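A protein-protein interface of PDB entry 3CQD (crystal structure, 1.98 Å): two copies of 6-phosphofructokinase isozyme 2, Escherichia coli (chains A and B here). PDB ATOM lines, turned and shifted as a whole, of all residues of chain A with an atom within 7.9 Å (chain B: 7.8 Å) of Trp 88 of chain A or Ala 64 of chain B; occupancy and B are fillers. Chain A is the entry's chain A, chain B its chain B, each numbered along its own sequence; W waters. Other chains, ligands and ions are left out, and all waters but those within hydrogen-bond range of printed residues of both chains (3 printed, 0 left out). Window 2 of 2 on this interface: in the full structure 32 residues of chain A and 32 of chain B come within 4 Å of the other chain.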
ATOM      1  N   PRO A  11      18.150  12.050  23.761  1.00  0.00           N
ATOM      2  CA  PRO A  11      17.152  13.034  23.408  1.00  0.00           C
ATOM      3  C   PRO A  11      17.658  14.028  22.354  1.00  0.00           C
ATOM      4  O   PRO A  11      18.841  14.037  22.014  1.00  0.00           O
ATOM      5  CB  PRO A  11      16.883  13.741  24.735  1.00  0.00           C
ATOM      6  CG  PRO A  11      18.138  13.646  25.468  1.00  0.00           C
ATOM      7  CD  PRO A  11      18.818  12.380  25.033  1.00  0.00           C
ATOM      8  N   SER A  12      16.761  14.843  21.826  1.00  0.00           N
ATOM      9  CA  SER A  12      17.202  15.916  20.951  1.00  0.00           C
ATOM     10  C   SER A  12      16.325  17.150  21.013  1.00  0.00           C
ATOM     11  O   SER A  12      15.164  17.090  21.417  1.00  0.00           O
ATOM     12  CB  SER A  12      17.363  15.415  19.499  1.00  0.00           C
ATOM     13  OG  SER A  12      16.150  14.898  19.013  1.00  0.00           O
ATOM     14  N   LEU A  13      16.908  18.286  20.643  1.00  0.00           N
ATOM     15  CA  LEU A  13      16.123  19.478  20.358  1.00  0.00           C
ATOM     16  C   LEU A  13      16.022  19.569  18.845  1.00  0.00           C
ATOM     17  O   LEU A  13      16.968  19.968  18.188  1.00  0.00           O
ATOM     18  CB  LEU A  13      16.800  20.732  20.914  1.00  0.00           C
ATOM     19  CG  LEU A  13      15.941  21.990  20.730  1.00  0.00           C
ATOM     20  CD1 LEU A  13      14.709  21.949  21.664  1.00  0.00           C
ATOM     21  CD2 LEU A  13      16.737  23.270  20.930  1.00  0.00           C
ATOM     22  N   PRO A  60      19.183  12.941  29.699  1.00  0.00           N
ATOM     23  CA  PRO A  60      20.285  13.859  29.785  1.00  0.00           C
ATOM     24  C   PRO A  60      19.974  15.146  29.010  1.00  0.00           C
ATOM     25  O   PRO A  60      19.378  15.109  27.928  1.00  0.00           O
ATOM     26  CB  PRO A  60      21.420  13.090  29.124  1.00  0.00           C
ATOM     27  CG  PRO A  60      20.740  12.196  28.152  1.00  0.00           C
ATOM     28  CD  PRO A  60      19.479  11.804  28.803  1.00  0.00           C
ATOM     29  N   ALA A  61      20.334  16.277  29.591  1.00  0.00           N
ATOM     30  CA  ALA A  61      20.128  17.557  28.936  1.00  0.00           C
ATOM     31  C   ALA A  61      21.436  18.324  29.053  1.00  0.00           C
ATOM     32  O   ALA A  61      22.013  18.408  30.123  1.00  0.00           O
ATOM     33  CB  ALA A  61      18.975  18.308  29.587  1.00  0.00           C
ATOM     34  N   GLY A  62      21.932  18.825  27.930  1.00  0.00           N
ATOM     35  CA  GLY A  62      23.151  19.603  27.938  1.00  0.00           C
ATOM     36  C   GLY A  62      22.993  20.914  27.216  1.00  0.00           C
ATOM     37  O   GLY A  62      22.400  20.980  26.129  1.00  0.00           O
ATOM     38  N   GLY A  63      23.498  21.964  27.853  1.00  0.00           N
ATOM     39  CA  GLY A  63      23.625  23.276  27.240  1.00  0.00           C
ATOM     40  C   GLY A  63      22.301  23.960  27.006  1.00  0.00           C
ATOM     41  O   GLY A  63      21.275  23.543  27.537  1.00  0.00           O
ATOM     42  N   ALA A  64      22.336  25.009  26.199  1.00  0.00           N
ATOM     43  CA  ALA A  64      21.148  25.790  25.917  1.00  0.00           C
ATOM     44  C   ALA A  64      20.103  25.008  25.112  1.00  0.00           C
ATOM     45  O   ALA A  64      18.906  25.228  25.272  1.00  0.00           O
ATOM     46  CB  ALA A  64      21.520  27.103  25.226  1.00  0.00           C
ATOM     47  N   THR A  65      20.549  24.086  24.261  1.00  0.00           N
ATOM     48  CA  THR A  65      19.613  23.215  23.547  1.00  0.00           C
ATOM     49  C   THR A  65      18.875  22.276  24.524  1.00  0.00           C
ATOM     50  O   THR A  65      17.661  22.099  24.427  1.00  0.00           O
ATOM     51  CB  THR A  65      20.302  22.389  22.459  1.00  0.00           C
ATOM     52  OG1 THR A  65      21.411  21.698  23.038  1.00  0.00           O
ATOM     53  CG2 THR A  65      20.771  23.275  21.297  1.00  0.00           C
ATOM     54  N   GLY A  66      19.612  21.684  25.464  1.00  0.00           N
ATOM     55  CA  GLY A  66      19.000  20.898  26.553  1.00  0.00           C
ATOM     56  C   GLY A  66      18.003  21.694  27.385  1.00  0.00           C
ATOM     57  O   GLY A  66      16.934  21.187  27.742  1.00  0.00           O
ATOM     58  N   GLU A  84      22.219  16.693  34.020  1.00  0.00           N
ATOM     59  CA  GLU A  84      23.047  17.615  33.270  1.00  0.00           C
ATOM     60  C   GLU A  84      24.179  16.875  32.589  1.00  0.00           C
ATOM     61  O   GLU A  84      24.903  16.113  33.222  1.00  0.00           O
ATOM     62  CB  GLU A  84      23.564  18.753  34.153  1.00  0.00           C
ATOM     63  CG  GLU A  84      22.588  19.909  34.217  1.00  0.00           C
ATOM     64  CD  GLU A  84      22.235  20.439  32.833  1.00  0.00           C
ATOM     65  OE1 GLU A  84      23.173  20.662  32.023  1.00  0.00           O
ATOM     66  OE2 GLU A  84      21.025  20.620  32.545  1.00  0.00           O
ATOM     67  N   ALA A  85      24.292  17.068  31.281  1.00  0.00           N
ATOM     68  CA  ALA A  85      25.337  16.391  30.529  1.00  0.00           C
ATOM     69  C   ALA A  85      26.318  17.400  29.974  1.00  0.00           C
ATOM     70  O   ALA A  85      25.938  18.516  29.595  1.00  0.00           O
ATOM     71  CB  ALA A  85      24.747  15.536  29.424  1.00  0.00           C
ATOM     72  N   LYS A  86      27.582  16.999  29.943  1.00  0.00           N
ATOM     73  CA  LYS A  86      28.675  17.823  29.431  1.00  0.00           C
ATOM     74  C   LYS A  86      28.441  18.215  27.978  1.00  0.00           C
ATOM     75  O   LYS A  86      28.491  19.379  27.620  1.00  0.00           O
ATOM     76  CB  LYS A  86      30.009  17.088  29.591  1.00  0.00           C
ATOM     77  CG  LYS A  86      30.609  17.172  30.993  1.00  0.00           C
ATOM     78  CD  LYS A  86      31.321  18.501  31.232  1.00  0.00           C
ATOM     79  CE  LYS A  86      31.964  18.556  32.611  1.00  0.00           C
ATOM     80  NZ  LYS A  86      30.960  18.620  33.712  1.00  0.00           N
ATOM     81  N   ASP A  87      28.163  17.220  27.154  1.00  0.00           N
ATOM     82  CA  ASP A  87      27.853  17.404  25.748  1.00  0.00           C
ATOM     83  C   ASP A  87      26.441  17.981  25.507  1.00  0.00           C
ATOM     84  O   ASP A  87      25.448  17.458  26.027  1.00  0.00           O
ATOM     85  CB  ASP A  87      28.007  16.061  25.038  1.00  0.00           C
ATOM     86  CG  ASP A  87      28.185  16.207  23.548  1.00  0.00           C
ATOM     87  OD1 ASP A  87      28.528  17.327  23.093  1.00  0.00           O
ATOM     88  OD2 ASP A  87      27.973  15.201  22.831  1.00  0.00           O
ATOM     89  N   TRP A  88      26.356  19.053  24.713  1.00  0.00           N
ATOM     90  CA  TRP A  88      25.073  19.738  24.479  1.00  0.00           C
ATOM     91  C   TRP A  88      24.081  18.849  23.735  1.00  0.00           C
ATOM     92  O   TRP A  88      24.450  18.086  22.831  1.00  0.00           O
ATOM     93  CB  TRP A  88      25.240  21.096  23.762  1.00  0.00           C
ATOM     94  CG  TRP A  88      25.505  21.000  22.269  1.00  0.00           C
ATOM     95  CD1 TRP A  88      24.567  20.877  21.260  1.00  0.00           C
ATOM     96  CD2 TRP A  88      26.780  21.009  21.624  1.00  0.00           C
ATOM     97  NE1 TRP A  88      25.189  20.803  20.038  1.00  0.00           N
ATOM     98  CE2 TRP A  88      26.547  20.885  20.230  1.00  0.00           C
ATOM     99  CE3 TRP A  88      28.101  21.102  22.086  1.00  0.00           C
ATOM    100  CZ2 TRP A  88      27.586  20.859  19.299  1.00  0.00           C
ATOM    101  CZ3 TRP A  88      29.139  21.078  21.153  1.00  0.00           C
ATOM    102  CH2 TRP A  88      28.871  20.953  19.778  1.00  0.00           C
ATOM    103  N   THR A  89      22.822  18.955  24.143  1.00  0.00           N
ATOM    104  CA  THR A  89      21.735  18.247  23.506  1.00  0.00           C
ATOM    105  C   THR A  89      21.729  18.491  22.003  1.00  0.00           C
ATOM    106  O   THR A  89      21.658  19.630  21.529  1.00  0.00           O
ATOM    107  CB  THR A  89      20.395  18.640  24.113  1.00  0.00           C
ATOM    108  OG1 THR A  89      20.412  18.337  25.515  1.00  0.00           O
ATOM    109  CG2 THR A  89      19.251  17.891  23.423  1.00  0.00           C
ATOM    110  N   ARG A  90      21.812  17.398  21.263  1.00  0.00           N
ATOM    111  CA  ARG A  90      21.951  17.473  19.828  1.00  0.00           C
ATOM    112  C   ARG A  90      20.625  17.801  19.151  1.00  0.00           C
ATOM    113  O   ARG A  90      19.564  17.743  19.769  1.00  0.00           O
ATOM    114  CB  ARG A  90      22.571  16.181  19.296  1.00  0.00           C
ATOM    115  CG  ARG A  90      24.023  15.985  19.703  1.00  0.00           C
ATOM    116  CD  ARG A  90      24.922  17.030  19.071  1.00  0.00           C
ATOM    117  NE  ARG A  90      26.326  16.653  19.123  1.00  0.00           N
ATOM    118  CZ  ARG A  90      27.168  16.988  20.097  1.00  0.00           C
ATOM    119  NH1 ARG A  90      28.439  16.593  20.025  1.00  0.00           N
ATOM    120  NH2 ARG A  90      26.743  17.697  21.146  1.00  0.00           N
ATOM    121  N   GLN A  91      20.707  18.171  17.878  1.00  0.00           N
ATOM    122  CA  GLN A  91      19.569  18.663  17.149  1.00  0.00           C
ATOM    123  C   GLN A  91      19.381  17.874  15.883  1.00  0.00           C
ATOM    124  O   GLN A  91      20.298  17.771  15.069  1.00  0.00           O
ATOM    125  CB  GLN A  91      19.790  20.132  16.810  1.00  0.00           C
ATOM    126  CG  GLN A  91      20.134  20.961  18.039  1.00  0.00           C
ATOM    127  CD  GLN A  91      20.503  22.383  17.696  1.00  0.00           C
ATOM    128  OE1 GLN A  91      21.688  22.733  17.648  1.00  0.00           O
ATOM    129  NE2 GLN A  91      19.496  23.216  17.466  1.00  0.00           N
ATOM    130  N   PRO A 109      22.835  11.048  15.812  1.00  0.00           N
ATOM    131  CA  PRO A 109      22.866  10.493  17.174  1.00  0.00           C
ATOM    132  C   PRO A 109      22.597  11.557  18.245  1.00  0.00           C
ATOM    133  O   PRO A 109      22.780  12.760  17.998  1.00  0.00           O
ATOM    134  CB  PRO A 109      24.296   9.961  17.320  1.00  0.00           C
ATOM    135  CG  PRO A 109      24.832   9.844  15.875  1.00  0.00           C
ATOM    136  CD  PRO A 109      24.125  10.909  15.105  1.00  0.00           C
ATOM    137  N   GLY A 110      22.166  11.113  19.423  1.00  0.00           N
ATOM    138  CA  GLY A 110      22.062  12.014  20.567  1.00  0.00           C
ATOM    139  C   GLY A 110      23.453  12.467  20.972  1.00  0.00           C
ATOM    140  O   GLY A 110      24.446  11.874  20.556  1.00  0.00           O
ATOM    141  N   ALA A 111      23.528  13.528  21.768  1.00  0.00           N
ATOM    142  CA  ALA A 111      24.784  13.939  22.392  1.00  0.00           C
ATOM    143  C   ALA A 111      25.458  12.753  23.090  1.00  0.00           C
ATOM    144  O   ALA A 111      24.785  11.787  23.490  1.00  0.00           O
ATOM    145  CB  ALA A 111      24.533  15.055  23.386  1.00  0.00           C
ATOM    146  N   ALA A 112      26.779  12.822  23.245  1.00  0.00           N
ATOM    147  CA  ALA A 112      27.494  11.774  23.979  1.00  0.00           C
ATOM    148  C   ALA A 112      27.067  11.791  25.439  1.00  0.00           C
ATOM    149  O   ALA A 112      26.687  12.840  25.991  1.00  0.00           O
ATOM    150  CB  ALA A 112      29.007  11.947  23.872  1.00  0.00           C
ATOM    151  N   LEU B  13      27.553  26.909  13.544  1.00  0.00           N
ATOM    152  CA  LEU B  13      28.380  25.748  13.697  1.00  0.00           C
ATOM    153  C   LEU B  13      27.655  24.672  12.929  1.00  0.00           C
ATOM    154  O   LEU B  13      26.663  24.162  13.387  1.00  0.00           O
ATOM    155  CB  LEU B  13      28.552  25.365  15.168  1.00  0.00           C
ATOM    156  CG  LEU B  13      29.416  24.119  15.368  1.00  0.00           C
ATOM    157  CD1 LEU B  13      30.898  24.468  15.199  1.00  0.00           C
ATOM    158  CD2 LEU B  13      29.131  23.510  16.729  1.00  0.00           C
ATOM    159  N   SER B  15      26.754  21.180  11.022  1.00  0.00           N
ATOM    160  CA  SER B  15      26.891  19.752  11.139  1.00  0.00           C
ATOM    161  C   SER B  15      26.997  19.156   9.738  1.00  0.00           C
ATOM    162  O   SER B  15      26.107  19.327   8.909  1.00  0.00           O
ATOM    163  CB  SER B  15      25.688  19.186  11.882  1.00  0.00           C
ATOM    164  OG  SER B  15      25.742  19.518  13.257  1.00  0.00           O
ATOM    165  N   PRO B  33      27.742  13.973  13.367  1.00  0.00           N
ATOM    166  CA  PRO B  33      28.207  15.068  12.538  1.00  0.00           C
ATOM    167  C   PRO B  33      29.661  15.416  12.772  1.00  0.00           C
ATOM    168  O   PRO B  33      30.193  15.235  13.876  1.00  0.00           O
ATOM    169  CB  PRO B  33      27.317  16.240  12.974  1.00  0.00           C
ATOM    170  CG  PRO B  33      26.922  15.910  14.371  1.00  0.00           C
ATOM    171  CD  PRO B  33      26.723  14.417  14.336  1.00  0.00           C
ATOM    172  N   PHE B  35      31.637  18.788  12.787  1.00  0.00           N
ATOM    173  CA  PHE B  35      31.326  20.205  12.863  1.00  0.00           C
ATOM    174  C   PHE B  35      32.265  21.029  12.009  1.00  0.00           C
ATOM    175  O   PHE B  35      33.457  20.741  11.884  1.00  0.00           O
ATOM    176  CB  PHE B  35      31.231  20.708  14.309  1.00  0.00           C
ATOM    177  CG  PHE B  35      30.210  19.979  15.113  1.00  0.00           C
ATOM    178  CD1 PHE B  35      30.591  19.179  16.180  1.00  0.00           C
ATOM    179  CD2 PHE B  35      28.864  20.059  14.780  1.00  0.00           C
ATOM    180  CE1 PHE B  35      29.637  18.485  16.921  1.00  0.00           C
ATOM    181  CE2 PHE B  35      27.910  19.375  15.503  1.00  0.00           C
ATOM    182  CZ  PHE B  35      28.296  18.582  16.582  1.00  0.00           C
ATOM    183  N   ALA B  61      29.406  34.638  19.356  1.00  0.00           N
ATOM    184  CA  ALA B  61      29.458  33.212  19.638  1.00  0.00           C
ATOM    185  C   ALA B  61      28.642  32.972  20.886  1.00  0.00           C
ATOM    186  O   ALA B  61      28.783  33.691  21.870  1.00  0.00           O
ATOM    187  CB  ALA B  61      30.891  32.754  19.821  1.00  0.00           C
ATOM    188  N   GLY B  62      27.765  31.974  20.833  1.00  0.00           N
ATOM    189  CA  GLY B  62      26.848  31.714  21.933  1.00  0.00           C
ATOM    190  C   GLY B  62      26.789  30.235  22.239  1.00  0.00           C
ATOM    191  O   GLY B  62      26.645  29.412  21.338  1.00  0.00           O
ATOM    192  N   GLY B  63      26.959  29.902  23.512  1.00  0.00           N
ATOM    193  CA  GLY B  63      26.858  28.530  23.979  1.00  0.00           C
ATOM    194  C   GLY B  63      28.020  27.648  23.586  1.00  0.00           C
ATOM    195  O   GLY B  63      29.002  28.111  23.012  1.00  0.00           O
ATOM    196  N   ALA B  64      27.882  26.366  23.902  1.00  0.00           N
ATOM    197  CA  ALA B  64      28.845  25.340  23.513  1.00  0.00           C
ATOM    198  C   ALA B  64      29.046  25.250  22.001  1.00  0.00           C
ATOM    199  O   ALA B  64      30.111  24.860  21.544  1.00  0.00           O
ATOM    200  CB  ALA B  64      28.419  23.992  24.078  1.00  0.00           C
ATOM    201  N   THR B  65      28.028  25.612  21.223  1.00  0.00           N
ATOM    202  CA  THR B  65      28.147  25.586  19.769  1.00  0.00           C
ATOM    203  C   THR B  65      29.064  26.741  19.346  1.00  0.00           C
ATOM    204  O   THR B  65      29.962  26.572  18.514  1.00  0.00           O
ATOM    205  CB  THR B  65      26.771  25.683  19.046  1.00  0.00           C
ATOM    206  OG1 THR B  65      26.022  26.785  19.576  1.00  0.00           O
ATOM    207  CG2 THR B  65      25.964  24.402  19.207  1.00  0.00           C
ATOM    208  N   GLY B  66      28.837  27.912  19.937  1.00  0.00           N
ATOM    209  CA  GLY B  66      29.735  29.047  19.768  1.00  0.00           C
ATOM    210  C   GLY B  66      31.144  28.670  20.185  1.00  0.00           C
ATOM    211  O   GLY B  66      32.103  28.943  19.469  1.00  0.00           O
ATOM    212  N   GLU B  67      31.267  28.014  21.336  1.00  0.00           N
ATOM    213  CA  GLU B  67      32.583  27.617  21.828  1.00  0.00           C
ATOM    214  C   GLU B  67      33.297  26.694  20.856  1.00  0.00           C
ATOM    215  O   GLU B  67      34.485  26.882  20.582  1.00  0.00           O
ATOM    216  CB  GLU B  67      32.476  26.961  23.193  1.00  0.00           C
ATOM    217  CG  GLU B  67      31.851  27.875  24.196  1.00  0.00           C
ATOM    218  CD  GLU B  67      32.091  27.443  25.611  1.00  0.00           C
ATOM    219  OE1 GLU B  67      31.823  28.276  26.501  1.00  0.00           O
ATOM    220  OE2 GLU B  67      32.542  26.289  25.830  1.00  0.00           O
ATOM    221  N   HIS B  68      32.565  25.720  20.320  1.00  0.00           N
ATOM    222  CA  HIS B  68      33.138  24.785  19.362  1.00  0.00           C
ATOM    223  C   HIS B  68      33.530  25.486  18.062  1.00  0.00           C
ATOM    224  O   HIS B  68      34.548  25.160  17.470  1.00  0.00           O
ATOM    225  CB  HIS B  68      32.191  23.616  19.095  1.00  0.00           C
ATOM    226  CG  HIS B  68      32.873  22.429  18.495  1.00  0.00           C
ATOM    227  ND1 HIS B  68      33.706  21.608  19.224  1.00  0.00           N
ATOM    228  CD2 HIS B  68      32.861  21.931  17.234  1.00  0.00           C
ATOM    229  CE1 HIS B  68      34.173  20.651  18.438  1.00  0.00           C
ATOM    230  NE2 HIS B  68      33.676  20.825  17.226  1.00  0.00           N
ATOM    231  N   LEU B  69      32.722  26.461  17.640  1.00  0.00           N
ATOM    232  CA  LEU B  69      33.046  27.289  16.480  1.00  0.00           C
ATOM    233  C   LEU B  69      34.400  27.977  16.667  1.00  0.00           C
ATOM    234  O   LEU B  69      35.271  27.911  15.798  1.00  0.00           O
ATOM    235  CB  LEU B  69      31.937  28.325  16.226  1.00  0.00           C
ATOM    236  CG  LEU B  69      32.130  29.315  15.070  1.00  0.00           C
ATOM    237  CD1 LEU B  69      32.409  28.599  13.735  1.00  0.00           C
ATOM    238  CD2 LEU B  69      30.921  30.210  14.941  1.00  0.00           C
ATOM    239  N   VAL B  70      34.564  28.625  17.816  1.00  0.00           N
ATOM    240  CA  VAL B  70      35.803  29.304  18.164  1.00  0.00           C
ATOM    241  C   VAL B  70      36.952  28.293  18.181  1.00  0.00           C
ATOM    242  O   VAL B  70      38.018  28.546  17.613  1.00  0.00           O
ATOM    243  CB  VAL B  70      35.658  30.045  19.517  1.00  0.00           C
ATOM    244  CG1 VAL B  70      36.998  30.617  19.994  1.00  0.00           C
ATOM    245  CG2 VAL B  70      34.606  31.144  19.392  1.00  0.00           C
ATOM    246  N   SER B  71      36.695  27.133  18.788  1.00  0.00           N
ATOM    247  CA  SER B  71      37.657  26.044  18.853  1.00  0.00           C
ATOM    248  C   SER B  71      38.052  25.528  17.469  1.00  0.00           C
ATOM    249  O   SER B  71      39.211  25.198  17.246  1.00  0.00           O
ATOM    250  CB  SER B  71      37.109  24.909  19.724  1.00  0.00           C
ATOM    251  OG  SER B  71      37.860  23.734  19.532  1.00  0.00           O
ATOM    252  N   TRP B  88      22.338  30.879  21.436  1.00  0.00           N
ATOM    253  CA  TRP B  88      23.339  29.897  21.044  1.00  0.00           C
ATOM    254  C   TRP B  88      23.603  29.913  19.543  1.00  0.00           C
ATOM    255  O   TRP B  88      22.688  30.027  18.738  1.00  0.00           O
ATOM    256  CB  TRP B  88      22.981  28.483  21.556  1.00  0.00           C
ATOM    257  CG  TRP B  88      21.939  27.667  20.747  1.00  0.00           C
ATOM    258  CD1 TRP B  88      22.171  26.910  19.614  1.00  0.00           C
ATOM    259  CD2 TRP B  88      20.546  27.497  21.054  1.00  0.00           C
ATOM    260  NE1 TRP B  88      21.006  26.304  19.196  1.00  0.00           N
ATOM    261  CE2 TRP B  88      19.995  26.650  20.056  1.00  0.00           C
ATOM    262  CE3 TRP B  88      19.703  27.995  22.066  1.00  0.00           C
ATOM    263  CZ2 TRP B  88      18.644  26.291  20.041  1.00  0.00           C
ATOM    264  CZ3 TRP B  88      18.358  27.626  22.056  1.00  0.00           C
ATOM    265  CH2 TRP B  88      17.842  26.779  21.046  1.00  0.00           C
ATOM    266  N   THR B  89      24.876  29.815  19.191  1.00  0.00           N
ATOM    267  CA  THR B  89      25.282  29.753  17.803  1.00  0.00           C
ATOM    268  C   THR B  89      24.519  28.640  17.120  1.00  0.00           C
ATOM    269  O   THR B  89      24.551  27.496  17.558  1.00  0.00           O
ATOM    270  CB  THR B  89      26.778  29.511  17.693  1.00  0.00           C
ATOM    271  OG1 THR B  89      27.455  30.629  18.269  1.00  0.00           O
ATOM    272  CG2 THR B  89      27.187  29.320  16.229  1.00  0.00           C
ATOM    273  N   GLN B  91      22.961  26.103  14.057  1.00  0.00           N
ATOM    274  CA  GLN B  91      23.533  25.037  13.264  1.00  0.00           C
ATOM    275  C   GLN B  91      22.838  24.861  11.938  1.00  0.00           C
ATOM    276  O   GLN B  91      21.615  24.688  11.865  1.00  0.00           O
ATOM    277  CB  GLN B  91      23.516  23.737  14.060  1.00  0.00           C
ATOM    278  CG  GLN B  91      24.334  23.874  15.360  1.00  0.00           C
ATOM    279  CD  GLN B  91      24.761  22.556  15.935  1.00  0.00           C
ATOM    280  OE1 GLN B  91      23.935  21.764  16.395  1.00  0.00           O
ATOM    281  NE2 GLN B  91      26.062  22.305  15.921  1.00  0.00           N
HETATM  282  O   HOH W   1      20.338  25.275  15.344  1.00  0.00           O
HETATM  283  O   HOH W   2      23.407  19.100  16.826  1.00  0.00           O
HETATM  284  O   HOH W   3      25.178  25.927  25.333  1.00  0.00           O
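The side-chain amide oxygen (OE1) of Gln 91 of chain A lies close to the side-chain amide oxygen (OE1) of Gln 91 of chain B.
The backbone NH (N) of Leu 13 of chain A is in hydrogen-bond range of the backbone carbonyl oxygen (O) of Arg 90 of chain A (2.8 Å). OG1 of Thr 65 of chain A is in hydrogen-bond range of O of Gly 62 of chain A, 3.3 Å away. The side-chain hydroxyl (OG1) of Thr 65 of chain A lies within hydrogen-bond range of the backbone carbonyl oxygen (O) of Thr 89 of chain A, 2.6 Å away. The guanidinium group of Arg 90 of chain A lies within salt-bridge range of the side-chain carboxylate of Asp 87 of chain A, at 2.7 Å. The backbone carbonyl oxygen (O) of Gly 62 of chain B sits at hydrogen-bond distance from the side-chain hydroxyl (OG1) of Thr 65 of chain B. OG1 of Thr 65 of chain B sits at hydrogen-bond distance from O of Thr 89 of chain B (2.6 Å).
Trp 88 of chain B touches Leu 13 of chain A. Ala 64 of chain A touches Trp 88 of chain B (CB to CE3, 3.8 Å). Trp 88 of chain B touches Thr 65 of chain A. Leu 13 of chain B touches Trp 88 of chain A (CD2 to CH2, 3.99 Å). Trp 88 of chain A touches Phe 35 of chain B (CZ2 to CZ, 3.6 Å). Ala 64 of chain B touches Trp 88 of chain A (CB to CE3, 3.5 Å). Thr 65 of chain B touches Trp 88 of chain A (CG2 to CE2, 3.7 Å). Trp 88 of chain A touches Gln 91 of chain B. Phe 35 of chain B touches Arg 90 of chain A. NE2 of Gln 91 of chain A touches NE1 of Trp 88 of chain B (3.8 Å).
Of the printed residues of chain B, Leu 13 of chain A touches Trp 88. Of the printed residues of chain B, Trp 88 of chain A touches Leu 13, Phe 35, Ala 64, Thr 65 and Gln 91. Of the printed residues of chain B, Arg 90 of chain A touches Phe 35. Of the printed residues of chain B, Gln 91 of chain A touches Trp 88 and Gln 91. No residue of chain A comes within 4 Å of Gly 63 of chain B. Ala 64 of chain B touches just one residue of chain A: Trp 88. The nearest printed residue of chain B that does not touch Trp 88 of chain A is His 68 of chain B (4.3 Å).
Hydrophobic or aromatic side chains of chain B within 4 Å of the printed part of chain A: Leu 13, Phe 35, Ala 64 and Trp 88. Of the 22 printed residues of chain A, 6 touch a printed residue of chain B. Hydrophobic or aromatic side chains of chain A within 4 Å of the printed part of chain B: Leu 13, Ala 64 and Trp 88. Among the printed residues, 11 pairs touch across the chains. Among the printed residues, no Asp or Glu carboxylate lies within 4 Å of a Lys or Arg side-chain nitrogen of the other chain.
Leu 13 of chain A touches Trp 88 of chain B, and with the chains exchanged Trp 88 of chain A touches Leu 13 of chain B. Ala 64 of chain A touches Trp 88 of chain B, and with the chains exchanged Trp 88 of chain A touches Ala 64 of chain B. Trp 88 of chain A touches Gln 91 of chain B, and with the chains exchanged Gln 91 of chain A touches Trp 88 of chain B. Gln 91 of chain B touches its own counterpart, Gln 91 of chain A.
Water W2 bridges OE1 of Gln 91 of chain B (2.7 Å) and N of Gln 91 of chain A (3.0 Å). Water W1 bridges N of Gln 91 of chain B (3.0 Å) and NE2 of Gln 91 of chain A (3.1 Å). Water W3 lies within hydrogen-bond range of the backbone NH (N) of Ala 64 of chain B (3.1 Å) and the backbone NH (N) of Ala 64 of chain A (3.1 Å).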
